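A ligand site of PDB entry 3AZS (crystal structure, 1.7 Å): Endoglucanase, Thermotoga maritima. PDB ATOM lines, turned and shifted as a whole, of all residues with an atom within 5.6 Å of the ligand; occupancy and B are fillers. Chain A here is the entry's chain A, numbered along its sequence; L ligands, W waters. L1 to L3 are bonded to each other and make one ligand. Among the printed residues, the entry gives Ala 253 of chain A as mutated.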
ATOM      1  N   ASN A  20      21.194  12.486   2.645  1.00  0.00           N
ATOM      2  CA  ASN A  20      19.970  12.111   1.934  1.00  0.00           C
ATOM      3  C   ASN A  20      18.777  12.647   2.702  1.00  0.00           C
ATOM      4  O   ASN A  20      17.681  12.093   2.706  1.00  0.00           O
ATOM      5  CB  ASN A  20      19.870  10.587   1.734  1.00  0.00           C
ATOM      6  CG  ASN A  20      20.679  10.130   0.548  1.00  0.00           C
ATOM      7  OD1 ASN A  20      20.125   9.656  -0.458  1.00  0.00           O
ATOM      8  ND2 ASN A  20      21.972  10.312   0.627  1.00  0.00           N
ATOM      9  N   GLU A  23      19.632  17.969   2.106  1.00  0.00           N
ATOM     10  CA  GLU A  23      20.225  18.379   0.844  1.00  0.00           C
ATOM     11  C   GLU A  23      19.416  17.918  -0.373  1.00  0.00           C
ATOM     12  O   GLU A  23      19.741  18.260  -1.496  1.00  0.00           O
ATOM     13  CB  GLU A  23      21.735  18.008   0.762  1.00  0.00           C
ATOM     14  CG  GLU A  23      22.064  16.583   0.348  1.00  0.00           C
ATOM     15  CD  GLU A  23      21.853  15.524   1.426  1.00  0.00           C
ATOM     16  OE1 GLU A  23      21.097  15.733   2.408  1.00  0.00           O
ATOM     17  OE2 GLU A  23      22.434  14.432   1.255  1.00  0.00           O
ATOM     18  N   ASP A  29      12.658  13.557   0.685  1.00  0.00           N
ATOM     19  CA  ASP A  29      12.558  13.156  -0.724  1.00  0.00           C
ATOM     20  C   ASP A  29      13.538  12.054  -1.058  1.00  0.00           C
ATOM     21  O   ASP A  29      13.223  11.188  -1.867  1.00  0.00           O
ATOM     22  CB  ASP A  29      12.834  14.311  -1.680  1.00  0.00           C
ATOM     23  CG  ASP A  29      11.697  15.314  -1.768  1.00  0.00           C
ATOM     24  OD1 ASP A  29      10.567  15.039  -1.291  1.00  0.00           O
ATOM     25  OD2 ASP A  29      11.964  16.379  -2.342  1.00  0.00           O
ATOM     26  N   TRP A  30      14.716  12.096  -0.430  1.00  0.00           N
ATOM     27  CA  TRP A  30      15.755  11.120  -0.727  1.00  0.00           C
ATOM     28  C   TRP A  30      15.878  10.041   0.325  1.00  0.00           C
ATOM     29  O   TRP A  30      16.886   9.346   0.408  1.00  0.00           O
ATOM     30  CB  TRP A  30      17.091  11.844  -0.937  1.00  0.00           C
ATOM     31  CG  TRP A  30      17.137  12.685  -2.212  1.00  0.00           C
ATOM     32  CD1 TRP A  30      16.126  12.862  -3.151  1.00  0.00           C
ATOM     33  CD2 TRP A  30      18.247  13.434  -2.677  1.00  0.00           C
ATOM     34  NE1 TRP A  30      16.558  13.693  -4.161  1.00  0.00           N
ATOM     35  CE2 TRP A  30      17.856  14.058  -3.890  1.00  0.00           C
ATOM     36  CE3 TRP A  30      19.550  13.659  -2.190  1.00  0.00           C
ATOM     37  CZ2 TRP A  30      18.726  14.870  -4.617  1.00  0.00           C
ATOM     38  CZ3 TRP A  30      20.403  14.479  -2.917  1.00  0.00           C
ATOM     39  CH2 TRP A  30      19.994  15.068  -4.123  1.00  0.00           C
ATOM     40  N   GLY A  31      14.838   9.925   1.135  1.00  0.00           N
ATOM     41  CA  GLY A  31      14.760   8.835   2.099  1.00  0.00           C
ATOM     42  C   GLY A  31      14.972   9.057   3.563  1.00  0.00           C
ATOM     43  O   GLY A  31      14.653   8.198   4.368  1.00  0.00           O
ATOM     44  N   ARG A  51      27.533  16.148  10.612  1.00  0.00           N
ATOM     45  CA  ARG A  51      27.649  17.098   9.487  1.00  0.00           C
ATOM     46  C   ARG A  51      26.290  17.048   8.841  1.00  0.00           C
ATOM     47  O   ARG A  51      25.735  15.961   8.550  1.00  0.00           O
ATOM     48  CB  ARG A  51      28.756  16.693   8.488  1.00  0.00           C
ATOM     49  CG  ARG A  51      28.803  17.610   7.261  1.00  0.00           C
ATOM     50  CD  ARG A  51      30.083  17.350   6.502  1.00  0.00           C
ATOM     51  NE  ARG A  51      30.163  18.172   5.269  1.00  0.00           N
ATOM     52  CZ  ARG A  51      29.850  17.753   4.048  1.00  0.00           C
ATOM     53  NH1 ARG A  51      29.404  16.524   3.817  1.00  0.00           N
ATOM     54  NH2 ARG A  51      30.121  18.544   3.013  1.00  0.00           N
ATOM     55  N   HIS A  95      24.876  22.918   0.169  1.00  0.00           N
ATOM     56  CA  HIS A  95      25.066  21.671  -0.593  1.00  0.00           C
ATOM     57  C   HIS A  95      24.097  21.644  -1.773  1.00  0.00           C
ATOM     58  O   HIS A  95      22.968  22.118  -1.669  1.00  0.00           O
ATOM     59  CB  HIS A  95      24.715  20.545   0.382  1.00  0.00           C
ATOM     60  CG  HIS A  95      25.439  19.239   0.159  1.00  0.00           C
ATOM     61  ND1 HIS A  95      25.144  18.355  -0.861  1.00  0.00           N
ATOM     62  CD2 HIS A  95      26.383  18.632   0.922  1.00  0.00           C
ATOM     63  CE1 HIS A  95      25.878  17.253  -0.713  1.00  0.00           C
ATOM     64  NE2 HIS A  95      26.629  17.398   0.358  1.00  0.00           N
ATOM     65  N   HIS A  96      24.568  21.086  -2.873  1.00  0.00           N
ATOM     66  CA  HIS A  96      23.782  20.974  -4.090  1.00  0.00           C
ATOM     67  C   HIS A  96      23.238  22.268  -4.627  1.00  0.00           C
ATOM     68  O   HIS A  96      22.050  22.366  -4.912  1.00  0.00           O
ATOM     69  CB  HIS A  96      22.670  19.929  -3.929  1.00  0.00           C
ATOM     70  CG  HIS A  96      23.204  18.519  -3.829  1.00  0.00           C
ATOM     71  ND1 HIS A  96      22.587  17.519  -3.094  1.00  0.00           N
ATOM     72  CD2 HIS A  96      24.346  17.983  -4.329  1.00  0.00           C
ATOM     73  CE1 HIS A  96      23.350  16.422  -3.132  1.00  0.00           C
ATOM     74  NE2 HIS A  96      24.415  16.686  -3.877  1.00  0.00           N
ATOM     75  N   ASN A 135      29.781  22.853  -0.472  1.00  0.00           N
ATOM     76  CA  ASN A 135      30.131  21.458  -0.740  1.00  0.00           C
ATOM     77  C   ASN A 135      30.588  21.247  -2.172  1.00  0.00           C
ATOM     78  O   ASN A 135      29.906  21.649  -3.107  1.00  0.00           O
ATOM     79  CB  ASN A 135      28.877  20.580  -0.539  1.00  0.00           C
ATOM     80  CG  ASN A 135      29.167  19.105  -0.790  1.00  0.00           C
ATOM     81  OD1 ASN A 135      29.852  18.468  -0.007  1.00  0.00           O
ATOM     82  ND2 ASN A 135      28.655  18.576  -1.910  1.00  0.00           N
ATOM     83  N   GLU A 136      31.800  20.712  -2.321  1.00  0.00           N
ATOM     84  CA  GLU A 136      32.316  20.283  -3.628  1.00  0.00           C
ATOM     85  C   GLU A 136      32.213  21.189  -4.824  1.00  0.00           C
ATOM     86  O   GLU A 136      31.515  20.882  -5.789  1.00  0.00           O
ATOM     87  CB  GLU A 136      31.663  18.918  -3.967  1.00  0.00           C
ATOM     88  CG  GLU A 136      32.022  17.894  -2.856  1.00  0.00           C
ATOM     89  CD  GLU A 136      31.282  16.569  -2.922  1.00  0.00           C
ATOM     90  OE1 GLU A 136      30.350  16.431  -3.720  1.00  0.00           O
ATOM     91  OE2 GLU A 136      31.626  15.660  -2.125  1.00  0.00           O
ATOM     92  N   HIS A 196      37.093  15.512   0.560  1.00  0.00           N
ATOM     93  CA  HIS A 196      36.201  14.362   0.615  1.00  0.00           C
ATOM     94  C   HIS A 196      37.016  13.250  -0.002  1.00  0.00           C
ATOM     95  O   HIS A 196      37.725  13.474  -1.015  1.00  0.00           O
ATOM     96  CB  HIS A 196      34.938  14.694  -0.154  1.00  0.00           C
ATOM     97  CG  HIS A 196      34.157  15.789   0.515  1.00  0.00           C
ATOM     98  ND1 HIS A 196      33.038  16.364  -0.039  1.00  0.00           N
ATOM     99  CD2 HIS A 196      34.340  16.400   1.711  1.00  0.00           C
ATOM    100  CE1 HIS A 196      32.559  17.286   0.775  1.00  0.00           C
ATOM    101  NE2 HIS A 196      33.329  17.331   1.842  1.00  0.00           N
ATOM    102  N   TYR A 198      36.960   9.471  -1.505  1.00  0.00           N
ATOM    103  CA  TYR A 198      36.192   8.343  -2.010  1.00  0.00           C
ATOM    104  C   TYR A 198      37.058   7.482  -2.937  1.00  0.00           C
ATOM    105  O   TYR A 198      36.541   6.703  -3.740  1.00  0.00           O
ATOM    106  CB  TYR A 198      34.994   8.880  -2.776  1.00  0.00           C
ATOM    107  CG  TYR A 198      33.917   9.457  -1.911  1.00  0.00           C
ATOM    108  CD1 TYR A 198      33.064   8.613  -1.189  1.00  0.00           C
ATOM    109  CD2 TYR A 198      33.717  10.833  -1.831  1.00  0.00           C
ATOM    110  CE1 TYR A 198      32.021   9.140  -0.388  1.00  0.00           C
ATOM    111  CE2 TYR A 198      32.691  11.373  -1.032  1.00  0.00           C
ATOM    112  CZ  TYR A 198      31.842  10.512  -0.329  1.00  0.00           C
ATOM    113  OH  TYR A 198      30.754  10.989   0.403  1.00  0.00           O
ATOM    114  N   HIS A 205      32.026   3.883  -5.380  1.00  0.00           N
ATOM    115  CA  HIS A 205      30.848   4.252  -6.149  1.00  0.00           C
ATOM    116  C   HIS A 205      30.275   3.230  -7.120  1.00  0.00           C
ATOM    117  O   HIS A 205      29.491   3.519  -7.908  1.00  0.00           O
ATOM    118  CB  HIS A 205      30.992   5.640  -6.761  1.00  0.00           C
ATOM    119  CG  HIS A 205      30.823   6.755  -5.815  1.00  0.00           C
ATOM    120  ND1 HIS A 205      31.752   7.079  -4.886  1.00  0.00           N
ATOM    121  CD2 HIS A 205      29.846   7.661  -5.723  1.00  0.00           C
ATOM    122  CE1 HIS A 205      31.325   8.125  -4.229  1.00  0.00           C
ATOM    123  NE2 HIS A 205      30.168   8.508  -4.707  1.00  0.00           N
ATOM    124  N   TRP A 210      23.415   7.348  -9.656  1.00  0.00           N
ATOM    125  CA  TRP A 210      23.528   8.723 -10.122  1.00  0.00           C
ATOM    126  C   TRP A 210      24.870   9.016 -10.787  1.00  0.00           C
ATOM    127  O   TRP A 210      25.171  10.163 -11.153  1.00  0.00           O
ATOM    128  CB  TRP A 210      23.304   9.688  -8.934  1.00  0.00           C
ATOM    129  CG  TRP A 210      24.298   9.555  -7.819  1.00  0.00           C
ATOM    130  CD1 TRP A 210      25.451  10.263  -7.649  1.00  0.00           C
ATOM    131  CD2 TRP A 210      24.289   8.569  -6.785  1.00  0.00           C
ATOM    132  NE1 TRP A 210      26.168   9.780  -6.581  1.00  0.00           N
ATOM    133  CE2 TRP A 210      25.478   8.732  -6.037  1.00  0.00           C
ATOM    134  CE3 TRP A 210      23.386   7.553  -6.428  1.00  0.00           C
ATOM    135  CZ2 TRP A 210      25.788   7.906  -4.957  1.00  0.00           C
ATOM    136  CZ3 TRP A 210      23.701   6.736  -5.350  1.00  0.00           C
ATOM    137  CH2 TRP A 210      24.888   6.918  -4.625  1.00  0.00           C
ATOM    138  N   ALA A 253      33.680  13.850   4.299  1.00  0.00           N
ATOM    139  CA  ALA A 253      32.851  12.824   3.709  1.00  0.00           C
ATOM    140  C   ALA A 253      33.744  11.760   3.130  1.00  0.00           C
ATOM    141  O   ALA A 253      34.673  12.063   2.366  1.00  0.00           O
ATOM    142  CB  ALA A 253      31.963  13.411   2.581  1.00  0.00           C
ATOM    143  N   TRP A 286      30.298   9.166   5.497  1.00  0.00           N
ATOM    144  CA  TRP A 286      29.146   9.375   4.611  1.00  0.00           C
ATOM    145  C   TRP A 286      28.542   7.958   4.472  1.00  0.00           C
ATOM    146  O   TRP A 286      29.155   7.096   3.833  1.00  0.00           O
ATOM    147  CB  TRP A 286      29.625   9.864   3.240  1.00  0.00           C
ATOM    148  CG  TRP A 286      28.474  10.144   2.312  1.00  0.00           C
ATOM    149  CD1 TRP A 286      27.874   9.254   1.431  1.00  0.00           C
ATOM    150  CD2 TRP A 286      27.655  11.307   2.321  1.00  0.00           C
ATOM    151  NE1 TRP A 286      26.717   9.823   0.921  1.00  0.00           N
ATOM    152  CE2 TRP A 286      26.558  11.075   1.447  1.00  0.00           C
ATOM    153  CE3 TRP A 286      27.741  12.548   2.987  1.00  0.00           C
ATOM    154  CZ2 TRP A 286      25.553  12.023   1.229  1.00  0.00           C
ATOM    155  CZ3 TRP A 286      26.740  13.505   2.767  1.00  0.00           C
ATOM    156  CH2 TRP A 286      25.653  13.246   1.897  1.00  0.00           C
ATOM    157  N   SER A 290      21.393   6.006   5.016  1.00  0.00           N
ATOM    158  CA  SER A 290      20.873   5.843   3.671  1.00  0.00           C
ATOM    159  C   SER A 290      21.688   4.813   2.847  1.00  0.00           C
ATOM    160  O   SER A 290      22.101   3.778   3.407  1.00  0.00           O
ATOM    161  CB  SER A 290      20.821   7.210   2.992  1.00  0.00           C
ATOM    162  OG  SER A 290      20.193   7.125   1.721  1.00  0.00           O
ATOM    163  N   PHE A 292      24.723   4.638   1.832  1.00  0.00           N
ATOM    164  CA  PHE A 292      26.065   4.344   2.356  1.00  0.00           C
ATOM    165  C   PHE A 292      25.936   4.085   3.861  1.00  0.00           C
ATOM    166  O   PHE A 292      26.921   4.054   4.613  1.00  0.00           O
ATOM    167  CB  PHE A 292      27.007   5.567   2.164  1.00  0.00           C
ATOM    168  CG  PHE A 292      27.414   5.834   0.754  1.00  0.00           C
ATOM    169  CD1 PHE A 292      28.736   5.681   0.350  1.00  0.00           C
ATOM    170  CD2 PHE A 292      26.480   6.360  -0.168  1.00  0.00           C
ATOM    171  CE1 PHE A 292      29.141   6.065  -0.938  1.00  0.00           C
ATOM    172  CE2 PHE A 292      26.872   6.743  -1.435  1.00  0.00           C
ATOM    173  CZ  PHE A 292      28.213   6.605  -1.832  1.00  0.00           C
HETATM  174  C1  LIG L   1      29.486  13.474  -1.629  1.00  0.00           C
HETATM  175  C2  LIG L   1      28.350  14.375  -1.944  1.00  0.00           C
HETATM  176  C3  LIG L   1      27.012  13.765  -1.733  1.00  0.00           C
HETATM  177  C4  LIG L   1      26.855  12.464  -2.477  1.00  0.00           C
HETATM  178  C5  LIG L   1      28.022  11.547  -1.938  1.00  0.00           C
HETATM  179  C6  LIG L   1      28.085  10.183  -2.520  1.00  0.00           C
HETATM  180  O1  LIG L   1      29.508  13.314  -0.282  1.00  0.00           O
HETATM  181  O2  LIG L   1      28.499  14.685  -3.316  1.00  0.00           O
HETATM  182  O3  LIG L   1      25.963  14.705  -2.100  1.00  0.00           O
HETATM  183  O4  LIG L   1      25.650  11.821  -1.994  1.00  0.00           O
HETATM  184  O5  LIG L   1      29.311  12.147  -2.205  1.00  0.00           O
HETATM  185  O6  LIG L   1      28.154  10.160  -3.943  1.00  0.00           O
HETATM  186  C1  LG2 L   2      24.881  11.384  -3.044  1.00  0.00           C
HETATM  187  C2  LG2 L   2      23.673  10.576  -2.492  1.00  0.00           C
HETATM  188  C3  LG2 L   2      22.797  10.117  -3.634  1.00  0.00           C
HETATM  189  C4  LG2 L   2      22.311  11.289  -4.418  1.00  0.00           C
HETATM  190  C5  LG2 L   2      23.515  12.042  -4.970  1.00  0.00           C
HETATM  191  C6  LG2 L   2      23.126  13.231  -5.721  1.00  0.00           C
HETATM  192  O1  LG2 L   2      22.986  11.415  -1.581  1.00  0.00           O
HETATM  193  O2  LG2 L   2      21.717   9.347  -3.035  1.00  0.00           O
HETATM  194  O3  LG2 L   2      21.519  10.890  -5.565  1.00  0.00           O
HETATM  195  O4  LG2 L   2      24.355  12.470  -3.851  1.00  0.00           O
HETATM  196  O5  LG2 L   2      24.200  13.921  -6.286  1.00  0.00           O
HETATM  197  C1  LG3 L   3      20.158  11.063  -5.436  1.00  0.00           C
HETATM  198  C2  LG3 L   3      19.462  11.366  -6.791  1.00  0.00           C
HETATM  199  C3  LG3 L   3      17.976  11.491  -6.586  1.00  0.00           C
HETATM  200  C4  LG3 L   3      17.446  10.297  -5.935  1.00  0.00           C
HETATM  201  C5  LG3 L   3      18.162  10.059  -4.603  1.00  0.00           C
HETATM  202  C6  LG3 L   3      17.719   8.840  -3.922  1.00  0.00           C
HETATM  203  O1  LG3 L   3      19.766  10.329  -7.697  1.00  0.00           O
HETATM  204  O2  LG3 L   3      17.309  11.764  -7.906  1.00  0.00           O
HETATM  205  O3  LG3 L   3      16.007  10.431  -5.684  1.00  0.00           O
HETATM  206  O4  LG3 L   3      19.625   9.931  -4.826  1.00  0.00           O
HETATM  207  O5  LG3 L   3      18.462   8.531  -2.772  1.00  0.00           O
HETATM  208  O   HOH W   1      26.841  14.275  -5.480  1.00  0.00           O
HETATM  209  O   HOH W   2      24.125  14.297  -8.887  1.00  0.00           O
HETATM  210  O   HOH W   3      28.133  11.854  -6.193  1.00  0.00           O
HETATM  211  O   HOH W   4      20.177  11.275 -10.057  1.00  0.00           O
HETATM  212  O   HOH W   5      15.319   7.448  -7.043  1.00  0.00           O
HETATM  213  O   HOH W   6      14.581  12.173  -7.579  1.00  0.00           O
HETATM  214  O   HOH W   7      23.449  14.102  -1.235  1.00  0.00           O
HETATM  215  O   HOH W   8      29.525  15.817   1.066  1.00  0.00           O
HETATM  216  O   HOH W   9      17.687   6.620  -1.100  1.00  0.00           O
HETATM  217  O   HOH W  10      22.669   6.965  -1.480  1.00  0.00           O
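NE2 of His 205 sits at hydrogen-bond distance from O6 of LIG L1, 2.7 Å away. O2 of LIG L1 is in hydrogen-bond range of OE1 of Glu 136 (2.6 Å). O1 of LG2 L2 sits at hydrogen-bond distance from ND2 of Asn 20, 2.7 Å away. An oxygen (O6) of LIG L1 is in hydrogen-bond range of the indole nitrogen (NE1) of Trp 210, at 3.3 Å. An oxygen (O1) of LIG L1 lies within hydrogen-bond range of the side-chain hydroxyl (OH) of Tyr 198 (2.7 Å). An oxygen (O3) of LIG L1 lies within hydrogen-bond range of a ring nitrogen (NE2) of His 96 (3.1 Å).
The side-chain carboxylate of Glu 136 sits at hydrogen-bond distance from a ring nitrogen (ND1) of His 196 (2.6 Å). A ring nitrogen (ND1) of His 95 lies close to a ring nitrogen (ND1) of His 96. The backbone carbonyl oxygen (O) of Glu 23 lies within hydrogen-bond range of a ring nitrogen (ND1) of His 96 (3.3 Å). The side-chain amide nitrogen (ND2) of Asn 135 lies within hydrogen-bond range of the side-chain carboxylate (OE1) of Glu 136, at 3.3 Å. N of Asn 20 sits at hydrogen-bond distance from OE2 of Glu 23, 2.7 Å away. OD1 of Asn 20 lies close to OG of Ser 290 (3.3 Å). A ring nitrogen (NE2) of His 95 is in hydrogen-bond range of the side-chain amide nitrogen (ND2) of Asn 135 (3.3 Å). The side-chain amide oxygen (OD1) of Asn 20 lies close to the backbone carbonyl oxygen (O) of Trp 30 (3.4 Å).
CD1 of Trp 30 touches O3 of LG3 L3, 3.5 Å away. His 95 touches the ligand. CB of Ala 253 touches O1 of LIG L1, at 3.8 Å. CZ2 of Trp 286 touches O4 of LIG L1, 3.2 Å away. CZ of Phe 292 touches C6 of LIG L1, 3.6 Å away. Hydrophobic or aromatic side chains that line the ligand: Trp 30, His 95, His 96, Tyr 198, His 205, Trp 210, Ala 253, Trp 286 and Phe 292. Within 4 Å of the ligand: Asn 20, Trp 30, His 95, His 96, Glu 136, Tyr 198, His 205, Trp 210, Ala 253, Trp 286 and Phe 292.
Water W9 lies within hydrogen-bond range of O5 of LG3 L3 and O of Trp 30. Water W7 bridges the side-chain carboxylate of Glu 23 and an oxygen (O3) of LIG L1. Water W3 lies within hydrogen-bond range of an oxygen (O6) of LIG L1 (2.8 Å) and the indole nitrogen of Trp 210 (2.9 Å). Water W8 lies within hydrogen-bond range of NH1 of Arg 51 (2.8 Å), O1 of LIG L1 (2.8 Å), OD1 of Asn 135 (2.9 Å) and NE2 of His 95 (3.4 Å).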
